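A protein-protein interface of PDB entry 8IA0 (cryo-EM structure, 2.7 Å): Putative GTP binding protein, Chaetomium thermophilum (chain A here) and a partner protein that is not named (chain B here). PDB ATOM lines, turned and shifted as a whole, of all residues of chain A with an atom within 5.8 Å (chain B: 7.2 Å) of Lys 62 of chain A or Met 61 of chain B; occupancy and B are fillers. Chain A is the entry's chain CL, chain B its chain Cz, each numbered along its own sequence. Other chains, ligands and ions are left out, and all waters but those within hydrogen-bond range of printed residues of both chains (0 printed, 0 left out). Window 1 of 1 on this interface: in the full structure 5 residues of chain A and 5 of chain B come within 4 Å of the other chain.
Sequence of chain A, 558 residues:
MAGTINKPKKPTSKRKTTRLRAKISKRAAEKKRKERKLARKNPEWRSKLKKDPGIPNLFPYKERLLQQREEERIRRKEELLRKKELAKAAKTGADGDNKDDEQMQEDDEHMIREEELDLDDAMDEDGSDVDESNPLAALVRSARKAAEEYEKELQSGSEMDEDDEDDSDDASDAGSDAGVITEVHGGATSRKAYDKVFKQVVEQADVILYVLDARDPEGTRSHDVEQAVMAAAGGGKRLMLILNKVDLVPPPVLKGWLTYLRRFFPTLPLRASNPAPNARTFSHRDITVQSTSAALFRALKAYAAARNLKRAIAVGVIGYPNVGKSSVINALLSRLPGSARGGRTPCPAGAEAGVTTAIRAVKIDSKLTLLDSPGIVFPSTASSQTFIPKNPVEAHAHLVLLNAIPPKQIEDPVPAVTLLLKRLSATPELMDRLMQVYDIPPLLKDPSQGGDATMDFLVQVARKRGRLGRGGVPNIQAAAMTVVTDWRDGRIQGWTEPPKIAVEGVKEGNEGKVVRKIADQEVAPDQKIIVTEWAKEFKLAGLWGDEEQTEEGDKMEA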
ATOM      1  N   GLY A  54       0.090  10.789   0.730  1.00  0.00           N
ATOM      2  CA  GLY A  54      -0.774  11.843   0.242  1.00  0.00           C
ATOM      3  C   GLY A  54      -0.838  13.041   1.169  1.00  0.00           C
ATOM      4  O   GLY A  54      -0.162  13.130   2.194  1.00  0.00           O
ATOM      5  N   ILE A  55      -1.686  13.987   0.784  1.00  0.00           N
ATOM      6  CA  ILE A  55      -1.824  15.244   1.529  1.00  0.00           C
ATOM      7  C   ILE A  55      -2.505  14.968   2.863  1.00  0.00           C
ATOM      8  O   ILE A  55      -3.505  14.229   2.901  1.00  0.00           O
ATOM      9  CB  ILE A  55      -2.617  16.261   0.706  1.00  0.00           C
ATOM     10  CG1 ILE A  55      -2.124  16.271  -0.740  1.00  0.00           C
ATOM     11  CG2 ILE A  55      -2.502  17.646   1.313  1.00  0.00           C
ATOM     12  CD1 ILE A  55      -3.075  16.945  -1.698  1.00  0.00           C
ATOM     13  N   PRO A  56      -2.011  15.517   3.970  1.00  0.00           N
ATOM     14  CA  PRO A  56      -2.687  15.316   5.255  1.00  0.00           C
ATOM     15  C   PRO A  56      -4.056  15.973   5.282  1.00  0.00           C
ATOM     16  O   PRO A  56      -4.306  16.979   4.613  1.00  0.00           O
ATOM     17  CB  PRO A  56      -1.736  15.974   6.261  1.00  0.00           C
ATOM     18  CG  PRO A  56      -0.410  15.987   5.573  1.00  0.00           C
ATOM     19  CD  PRO A  56      -0.725  16.210   4.130  1.00  0.00           C
ATOM     20  N   ASN A  57      -4.950  15.385   6.078  1.00  0.00           N
ATOM     21  CA  ASN A  57      -6.326  15.866   6.136  1.00  0.00           C
ATOM     22  C   ASN A  57      -6.434  17.208   6.845  1.00  0.00           C
ATOM     23  O   ASN A  57      -7.323  18.004   6.523  1.00  0.00           O
ATOM     24  CB  ASN A  57      -7.214  14.831   6.824  1.00  0.00           C
ATOM     25  CG  ASN A  57      -7.822  13.848   5.848  1.00  0.00           C
ATOM     26  OD1 ASN A  57      -8.945  14.032   5.383  1.00  0.00           O
ATOM     27  ND2 ASN A  57      -7.077  12.799   5.526  1.00  0.00           N
ATOM     28  N   PHE A  59      -4.506  19.714   6.629  1.00  0.00           N
ATOM     29  CA  PHE A  59      -4.027  20.831   5.826  1.00  0.00           C
ATOM     30  C   PHE A  59      -5.219  21.661   5.369  1.00  0.00           C
ATOM     31  O   PHE A  59      -6.109  21.129   4.695  1.00  0.00           O
ATOM     32  CB  PHE A  59      -3.235  20.309   4.631  1.00  0.00           C
ATOM     33  CG  PHE A  59      -2.414  21.357   3.938  1.00  0.00           C
ATOM     34  CD1 PHE A  59      -1.537  22.152   4.652  1.00  0.00           C
ATOM     35  CD2 PHE A  59      -2.508  21.533   2.571  1.00  0.00           C
ATOM     36  CE1 PHE A  59      -0.778  23.110   4.013  1.00  0.00           C
ATOM     37  CE2 PHE A  59      -1.751  22.488   1.929  1.00  0.00           C
ATOM     38  CZ  PHE A  59      -0.886  23.277   2.650  1.00  0.00           C
ATOM     39  N   PRO A  60      -5.287  22.951   5.711  1.00  0.00           N
ATOM     40  CA  PRO A  60      -6.506  23.725   5.427  1.00  0.00           C
ATOM     41  C   PRO A  60      -6.809  23.904   3.951  1.00  0.00           C
ATOM     42  O   PRO A  60      -7.967  24.172   3.609  1.00  0.00           O
ATOM     43  CB  PRO A  60      -6.231  25.075   6.104  1.00  0.00           C
ATOM     44  CG  PRO A  60      -4.749  25.145   6.222  1.00  0.00           C
ATOM     45  CD  PRO A  60      -4.293  23.742   6.454  1.00  0.00           C
ATOM     46  N   TYR A  61      -5.825  23.766   3.066  1.00  0.00           N
ATOM     47  CA  TYR A  61      -6.021  24.007   1.641  1.00  0.00           C
ATOM     48  C   TYR A  61      -5.962  22.719   0.825  1.00  0.00           C
ATOM     49  O   TYR A  61      -5.382  22.693  -0.263  1.00  0.00           O
ATOM     50  CB  TYR A  61      -4.999  25.015   1.123  1.00  0.00           C
ATOM     51  CG  TYR A  61      -5.006  26.324   1.877  1.00  0.00           C
ATOM     52  CD1 TYR A  61      -6.192  26.997   2.118  1.00  0.00           C
ATOM     53  CD2 TYR A  61      -3.828  26.883   2.346  1.00  0.00           C
ATOM     54  CE1 TYR A  61      -6.206  28.192   2.805  1.00  0.00           C
ATOM     55  CE2 TYR A  61      -3.833  28.078   3.035  1.00  0.00           C
ATOM     56  CZ  TYR A  61      -5.024  28.728   3.259  1.00  0.00           C
ATOM     57  OH  TYR A  61      -5.035  29.918   3.945  1.00  0.00           O
ATOM     58  N   LYS A  62      -6.558  21.642   1.338  1.00  0.00           N
ATOM     59  CA  LYS A  62      -6.608  20.399   0.576  1.00  0.00           C
ATOM     60  C   LYS A  62      -7.621  20.490  -0.560  1.00  0.00           C
ATOM     61  O   LYS A  62      -7.483  19.799  -1.576  1.00  0.00           O
ATOM     62  CB  LYS A  62      -6.929  19.230   1.504  1.00  0.00           C
ATOM     63  CG  LYS A  62      -6.548  17.873   0.947  1.00  0.00           C
ATOM     64  CD  LYS A  62      -6.585  16.810   2.027  1.00  0.00           C
ATOM     65  CE  LYS A  62      -6.508  15.419   1.427  1.00  0.00           C
ATOM     66  NZ  LYS A  62      -6.257  14.378   2.459  1.00  0.00           N
ATOM     67  N   GLU A  63      -8.649  21.328  -0.403  1.00  0.00           N
ATOM     68  CA  GLU A  63      -9.588  21.569  -1.495  1.00  0.00           C
ATOM     69  C   GLU A  63      -8.889  22.189  -2.697  1.00  0.00           C
ATOM     70  O   GLU A  63      -9.006  21.694  -3.824  1.00  0.00           O
ATOM     71  CB  GLU A  63     -10.727  22.476  -1.025  1.00  0.00           C
ATOM     72  CG  GLU A  63     -12.040  21.769  -0.755  1.00  0.00           C
ATOM     73  CD  GLU A  63     -12.871  21.588  -2.009  1.00  0.00           C
ATOM     74  OE1 GLU A  63     -12.593  22.280  -3.012  1.00  0.00           O
ATOM     75  OE2 GLU A  63     -13.803  20.758  -1.993  1.00  0.00           O
ATOM     76  N   ARG A  64      -8.157  23.280  -2.474  1.00  0.00           N
ATOM     77  CA  ARG A  64      -7.537  23.992  -3.584  1.00  0.00           C
ATOM     78  C   ARG A  64      -6.424  23.168  -4.217  1.00  0.00           C
ATOM     79  O   ARG A  64      -6.230  23.207  -5.436  1.00  0.00           O
ATOM     80  CB  ARG A  64      -7.008  25.343  -3.105  1.00  0.00           C
ATOM     81  CG  ARG A  64      -8.053  26.183  -2.393  1.00  0.00           C
ATOM     82  CD  ARG A  64      -7.583  27.610  -2.172  1.00  0.00           C
ATOM     83  NE  ARG A  64      -6.162  27.678  -1.856  1.00  0.00           N
ATOM     84  CZ  ARG A  64      -5.568  28.727  -1.306  1.00  0.00           C
ATOM     85  NH1 ARG A  64      -6.245  29.820  -0.993  1.00  0.00           N
ATOM     86  NH2 ARG A  64      -4.261  28.679  -1.061  1.00  0.00           N
ATOM     87  N   LEU A  65      -5.684  22.414  -3.404  1.00  0.00           N
ATOM     88  CA  LEU A  65      -4.577  21.626  -3.934  1.00  0.00           C
ATOM     89  C   LEU A  65      -5.077  20.460  -4.778  1.00  0.00           C
ATOM     90  O   LEU A  65      -4.513  20.170  -5.840  1.00  0.00           O
ATOM     91  CB  LEU A  65      -3.694  21.130  -2.792  1.00  0.00           C
ATOM     92  CG  LEU A  65      -2.289  20.674  -3.178  1.00  0.00           C
ATOM     93  CD1 LEU A  65      -1.574  21.763  -3.958  1.00  0.00           C
ATOM     94  CD2 LEU A  65      -1.498  20.291  -1.940  1.00  0.00           C
ATOM     95  N   LEU A  66      -6.130  19.776  -4.324  1.00  0.00           N
ATOM     96  CA  LEU A  66      -6.689  18.683  -5.114  1.00  0.00           C
ATOM     97  C   LEU A  66      -7.357  19.193  -6.383  1.00  0.00           C
ATOM     98  O   LEU A  66      -7.245  18.558  -7.437  1.00  0.00           O
ATOM     99  CB  LEU A  66      -7.679  17.878  -4.277  1.00  0.00           C
ATOM    100  CG  LEU A  66      -7.062  16.952  -3.228  1.00  0.00           C
ATOM    101  CD1 LEU A  66      -8.132  16.103  -2.566  1.00  0.00           C
ATOM    102  CD2 LEU A  66      -5.991  16.077  -3.852  1.00  0.00           C
ATOM    103  N   GLN A  67      -8.055  20.328  -6.301  1.00  0.00           N
ATOM    104  CA  GLN A  67      -8.593  20.949  -7.507  1.00  0.00           C
ATOM    105  C   GLN A  67      -7.471  21.370  -8.445  1.00  0.00           C
ATOM    106  O   GLN A  67      -7.588  21.232  -9.668  1.00  0.00           O
ATOM    107  CB  GLN A  67      -9.462  22.151  -7.140  1.00  0.00           C
ATOM    108  CG  GLN A  67     -10.848  21.787  -6.641  1.00  0.00           C
ATOM    109  CD  GLN A  67     -11.743  22.998  -6.485  1.00  0.00           C
ATOM    110  OE1 GLN A  67     -11.411  24.093  -6.940  1.00  0.00           O
ATOM    111  NE2 GLN A  67     -12.888  22.809  -5.838  1.00  0.00           N
ATOM    112  N   ARG B  55     -17.088  21.050   9.643  1.00  0.00           N
ATOM    113  CA  ARG B  55     -17.553  19.676   9.494  1.00  0.00           C
ATOM    114  C   ARG B  55     -18.110  19.428   8.097  1.00  0.00           C
ATOM    115  O   ARG B  55     -17.880  18.364   7.511  1.00  0.00           O
ATOM    116  CB  ARG B  55     -18.600  19.353  10.561  1.00  0.00           C
ATOM    117  CG  ARG B  55     -18.565  17.906  11.030  1.00  0.00           C
ATOM    118  CD  ARG B  55     -19.915  17.443  11.553  1.00  0.00           C
ATOM    119  NE  ARG B  55     -20.328  18.185  12.738  1.00  0.00           N
ATOM    120  CZ  ARG B  55     -21.417  17.920  13.446  1.00  0.00           C
ATOM    121  NH1 ARG B  55     -22.229  16.929  13.118  1.00  0.00           N
ATOM    122  NH2 ARG B  55     -21.697  18.666  14.509  1.00  0.00           N
ATOM    123  N   GLN B  56     -18.847  20.396   7.546  1.00  0.00           N
ATOM    124  CA  GLN B  56     -19.357  20.253   6.186  1.00  0.00           C
ATOM    125  C   GLN B  56     -18.223  20.257   5.166  1.00  0.00           C
ATOM    126  O   GLN B  56     -18.247  19.488   4.199  1.00  0.00           O
ATOM    127  CB  GLN B  56     -20.358  21.364   5.880  1.00  0.00           C
ATOM    128  CG  GLN B  56     -21.502  21.453   6.874  1.00  0.00           C
ATOM    129  CD  GLN B  56     -22.486  22.551   6.533  1.00  0.00           C
ATOM    130  OE1 GLN B  56     -22.595  22.967   5.379  1.00  0.00           O
ATOM    131  NE2 GLN B  56     -23.211  23.028   7.537  1.00  0.00           N
ATOM    132  N   GLU B  57     -17.228  21.125   5.360  1.00  0.00           N
ATOM    133  CA  GLU B  57     -16.079  21.145   4.461  1.00  0.00           C
ATOM    134  C   GLU B  57     -15.287  19.846   4.550  1.00  0.00           C
ATOM    135  O   GLU B  57     -14.830  19.318   3.530  1.00  0.00           O
ATOM    136  CB  GLU B  57     -15.183  22.341   4.776  1.00  0.00           C
ATOM    137  CG  GLU B  57     -15.890  23.682   4.703  1.00  0.00           C
ATOM    138  CD  GLU B  57     -14.943  24.823   4.383  1.00  0.00           C
ATOM    139  OE1 GLU B  57     -13.833  24.551   3.880  1.00  0.00           O
ATOM    140  OE2 GLU B  57     -15.310  25.989   4.636  1.00  0.00           O
ATOM    141  N   GLN B  58     -15.106  19.324   5.765  1.00  0.00           N
ATOM    142  CA  GLN B  58     -14.427  18.042   5.922  1.00  0.00           C
ATOM    143  C   GLN B  58     -15.217  16.924   5.253  1.00  0.00           C
ATOM    144  O   GLN B  58     -14.631  15.987   4.698  1.00  0.00           O
ATOM    145  CB  GLN B  58     -14.206  17.743   7.406  1.00  0.00           C
ATOM    146  CG  GLN B  58     -13.741  16.327   7.700  1.00  0.00           C
ATOM    147  CD  GLN B  58     -12.261  16.135   7.441  1.00  0.00           C
ATOM    148  OE1 GLN B  58     -11.861  15.664   6.376  1.00  0.00           O
ATOM    149  NE2 GLN B  58     -11.436  16.502   8.415  1.00  0.00           N
ATOM    150  N   ALA B  59     -16.548  17.009   5.291  1.00  0.00           N
ATOM    151  CA  ALA B  59     -17.369  16.064   4.542  1.00  0.00           C
ATOM    152  C   ALA B  59     -17.127  16.199   3.045  1.00  0.00           C
ATOM    153  O   ALA B  59     -17.099  15.199   2.319  1.00  0.00           O
ATOM    154  CB  ALA B  59     -18.847  16.271   4.872  1.00  0.00           C
ATOM    155  N   ALA B  60     -16.956  17.433   2.564  1.00  0.00           N
ATOM    156  CA  ALA B  60     -16.614  17.641   1.161  1.00  0.00           C
ATOM    157  C   ALA B  60     -15.241  17.063   0.840  1.00  0.00           C
ATOM    158  O   ALA B  60     -15.025  16.533  -0.256  1.00  0.00           O
ATOM    159  CB  ALA B  60     -16.666  19.129   0.820  1.00  0.00           C
ATOM    160  N   MET B  61     -14.296  17.173   1.778  1.00  0.00           N
ATOM    161  CA  MET B  61     -12.993  16.540   1.602  1.00  0.00           C
ATOM    162  C   MET B  61     -13.143  15.041   1.384  1.00  0.00           C
ATOM    163  O   MET B  61     -12.621  14.483   0.412  1.00  0.00           O
ATOM    164  CB  MET B  61     -12.114  16.791   2.828  1.00  0.00           C
ATOM    165  CG  MET B  61     -10.739  17.359   2.536  1.00  0.00           C
ATOM    166  SD  MET B  61     -10.757  18.567   1.209  1.00  0.00           S
ATOM    167  CE  MET B  61     -11.352  19.984   2.128  1.00  0.00           C
ATOM    168  N   LYS B  62     -13.864  14.375   2.288  1.00  0.00           N
ATOM    169  CA  LYS B  62     -13.955  12.921   2.256  1.00  0.00           C
ATOM    170  C   LYS B  62     -14.656  12.437   0.996  1.00  0.00           C
ATOM    171  O   LYS B  62     -14.221  11.464   0.369  1.00  0.00           O
ATOM    172  CB  LYS B  62     -14.683  12.429   3.507  1.00  0.00           C
ATOM    173  CG  LYS B  62     -13.870  12.582   4.782  1.00  0.00           C
ATOM    174  CD  LYS B  62     -14.581  11.983   5.983  1.00  0.00           C
ATOM    175  CE  LYS B  62     -13.668  11.956   7.199  1.00  0.00           C
ATOM    176  NZ  LYS B  62     -14.276  11.219   8.339  1.00  0.00           N
ATOM    177  N   ALA B  63     -15.745  13.104   0.606  1.00  0.00           N
ATOM    178  CA  ALA B  63     -16.483  12.691  -0.583  1.00  0.00           C
ATOM    179  C   ALA B  63     -15.631  12.841  -1.837  1.00  0.00           C
ATOM    180  O   ALA B  63     -15.610  11.952  -2.696  1.00  0.00           O
ATOM    181  CB  ALA B  63     -17.774  13.499  -0.705  1.00  0.00           C
ATOM    182  N   LYS B  64     -14.922  13.965  -1.959  1.00  0.00           N
ATOM    183  CA  LYS B  64     -14.067  14.176  -3.122  1.00  0.00           C
ATOM    184  C   LYS B  64     -12.891  13.207  -3.128  1.00  0.00           C
ATOM    185  O   LYS B  64     -12.512  12.683  -4.181  1.00  0.00           O
ATOM    186  CB  LYS B  64     -13.575  15.622  -3.153  1.00  0.00           C
ATOM    187  CG  LYS B  64     -12.436  15.872  -4.123  1.00  0.00           C
ATOM    188  CD  LYS B  64     -12.675  17.131  -4.936  1.00  0.00           C
ATOM    189  CE  LYS B  64     -11.957  17.066  -6.272  1.00  0.00           C
ATOM    190  NZ  LYS B  64     -12.903  16.818  -7.395  1.00  0.00           N
ATOM    191  N   GLU B  65     -12.293  12.963  -1.960  1.00  0.00           N
ATOM    192  CA  GLU B  65     -11.194  12.008  -1.878  1.00  0.00           C
ATOM    193  C   GLU B  65     -11.674  10.587  -2.149  1.00  0.00           C
ATOM    194  O   GLU B  65     -10.991   9.814  -2.830  1.00  0.00           O
ATOM    195  CB  GLU B  65     -10.523  12.095  -0.508  1.00  0.00           C
ATOM    196  CG  GLU B  65      -9.229  11.305  -0.395  1.00  0.00           C
ATOM    197  CD  GLU B  65      -8.584  11.435   0.972  1.00  0.00           C
ATOM    198  OE1 GLU B  65      -9.155  12.130   1.838  1.00  0.00           O
ATOM    199  OE2 GLU B  65      -7.504  10.842   1.179  1.00  0.00           O
ATOM    200  N   ARG B  66     -12.845  10.223  -1.620  1.00  0.00           N
ATOM    201  CA  ARG B  66     -13.341   8.859  -1.781  1.00  0.00           C
ATOM    202  C   ARG B  66     -13.632   8.538  -3.241  1.00  0.00           C
ATOM    203  O   ARG B  66     -13.321   7.440  -3.716  1.00  0.00           O
ATOM    204  CB  ARG B  66     -14.592   8.648  -0.928  1.00  0.00           C
ATOM    205  CG  ARG B  66     -14.307   8.210   0.501  1.00  0.00           C
ATOM    206  CD  ARG B  66     -15.595   7.932   1.263  1.00  0.00           C
ATOM    207  NE  ARG B  66     -15.338   7.408   2.599  1.00  0.00           N
ATOM    208  CZ  ARG B  66     -16.283   7.104   3.479  1.00  0.00           C
ATOM    209  NH1 ARG B  66     -17.566   7.259   3.197  1.00  0.00           N
ATOM    210  NH2 ARG B  66     -15.931   6.634   4.672  1.00  0.00           N
ATOM    211  N   GLU B  67     -14.232   9.482  -3.971  1.00  0.00           N
ATOM    212  CA  GLU B  67     -14.562   9.222  -5.368  1.00  0.00           C
ATOM    213  C   GLU B  67     -13.308   9.168  -6.231  1.00  0.00           C
ATOM    214  O   GLU B  67     -13.271   8.450  -7.238  1.00  0.00           O
ATOM    215  CB  GLU B  67     -15.542  10.276  -5.887  1.00  0.00           C
ATOM    216  CG  GLU B  67     -15.025  11.705  -5.855  1.00  0.00           C
ATOM    217  CD  GLU B  67     -14.399  12.129  -7.168  1.00  0.00           C
ATOM    218  OE1 GLU B  67     -14.658  11.466  -8.194  1.00  0.00           O
ATOM    219  OE2 GLU B  67     -13.648  13.127  -7.175  1.00  0.00           O
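The side-chain amide oxygen (OE1) of Gln 58 of chain B lies close to the side-chain amide oxygen (OD1) of Asn 57 of chain A, at 3.5 Å.
The side-chain carboxylate (OE1) of Glu 65 of chain B is in salt-bridge range of the side-chain amino group (NZ) of Lys 62 of chain A (3.7 Å).
The side-chain amino group of Lys 62 of chain A is in hydrogen-bond range of the backbone carbonyl oxygen of Ile 55 of chain A, at 2.8 Å.
OE1 of Glu 63 of chain A lies within hydrogen-bond range of NE2 of Gln 67 of chain A, 2.9 Å away.
Met 61 of chain B touches Lys 62 of chain A.
CG of Glu 63 of chain A touches CE of Met 61 of chain B, 3.5 Å away.
Lys 62 of chain A touches just these residues of chain B: Met 61 and Glu 65.
Met 61 of chain B touches two residues of chain A.
Of the printed residues of chain B, Glu 63 of chain A touches Met 61 (3.5 Å).
Of the printed residues of chain B, Asn 57 of chain A touches Gln 58.
Leu 66 of chain A touches none of the printed residues of chain B.
The nearest residue of chain B that does not touch Lys 62 of chain A is Lys 64 of chain B (6.7 Å).
The nearest residue of chain A that does not touch Met 61 of chain B is Asn 57 of chain A (4.7 Å).
Printed residues of chain A that touch a printed residue of chain B: Asn 57, Lys 62 and Glu 63.
Of the 13 printed residues of chain B, 3 touch a printed residue of chain A.
Among the printed residues, Asp or Glu carboxylates within 4 Å of a Lys or Arg side-chain nitrogen of the other chain: Lys 62 of chain A with Glu 65 of chain B (3.7 Å).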
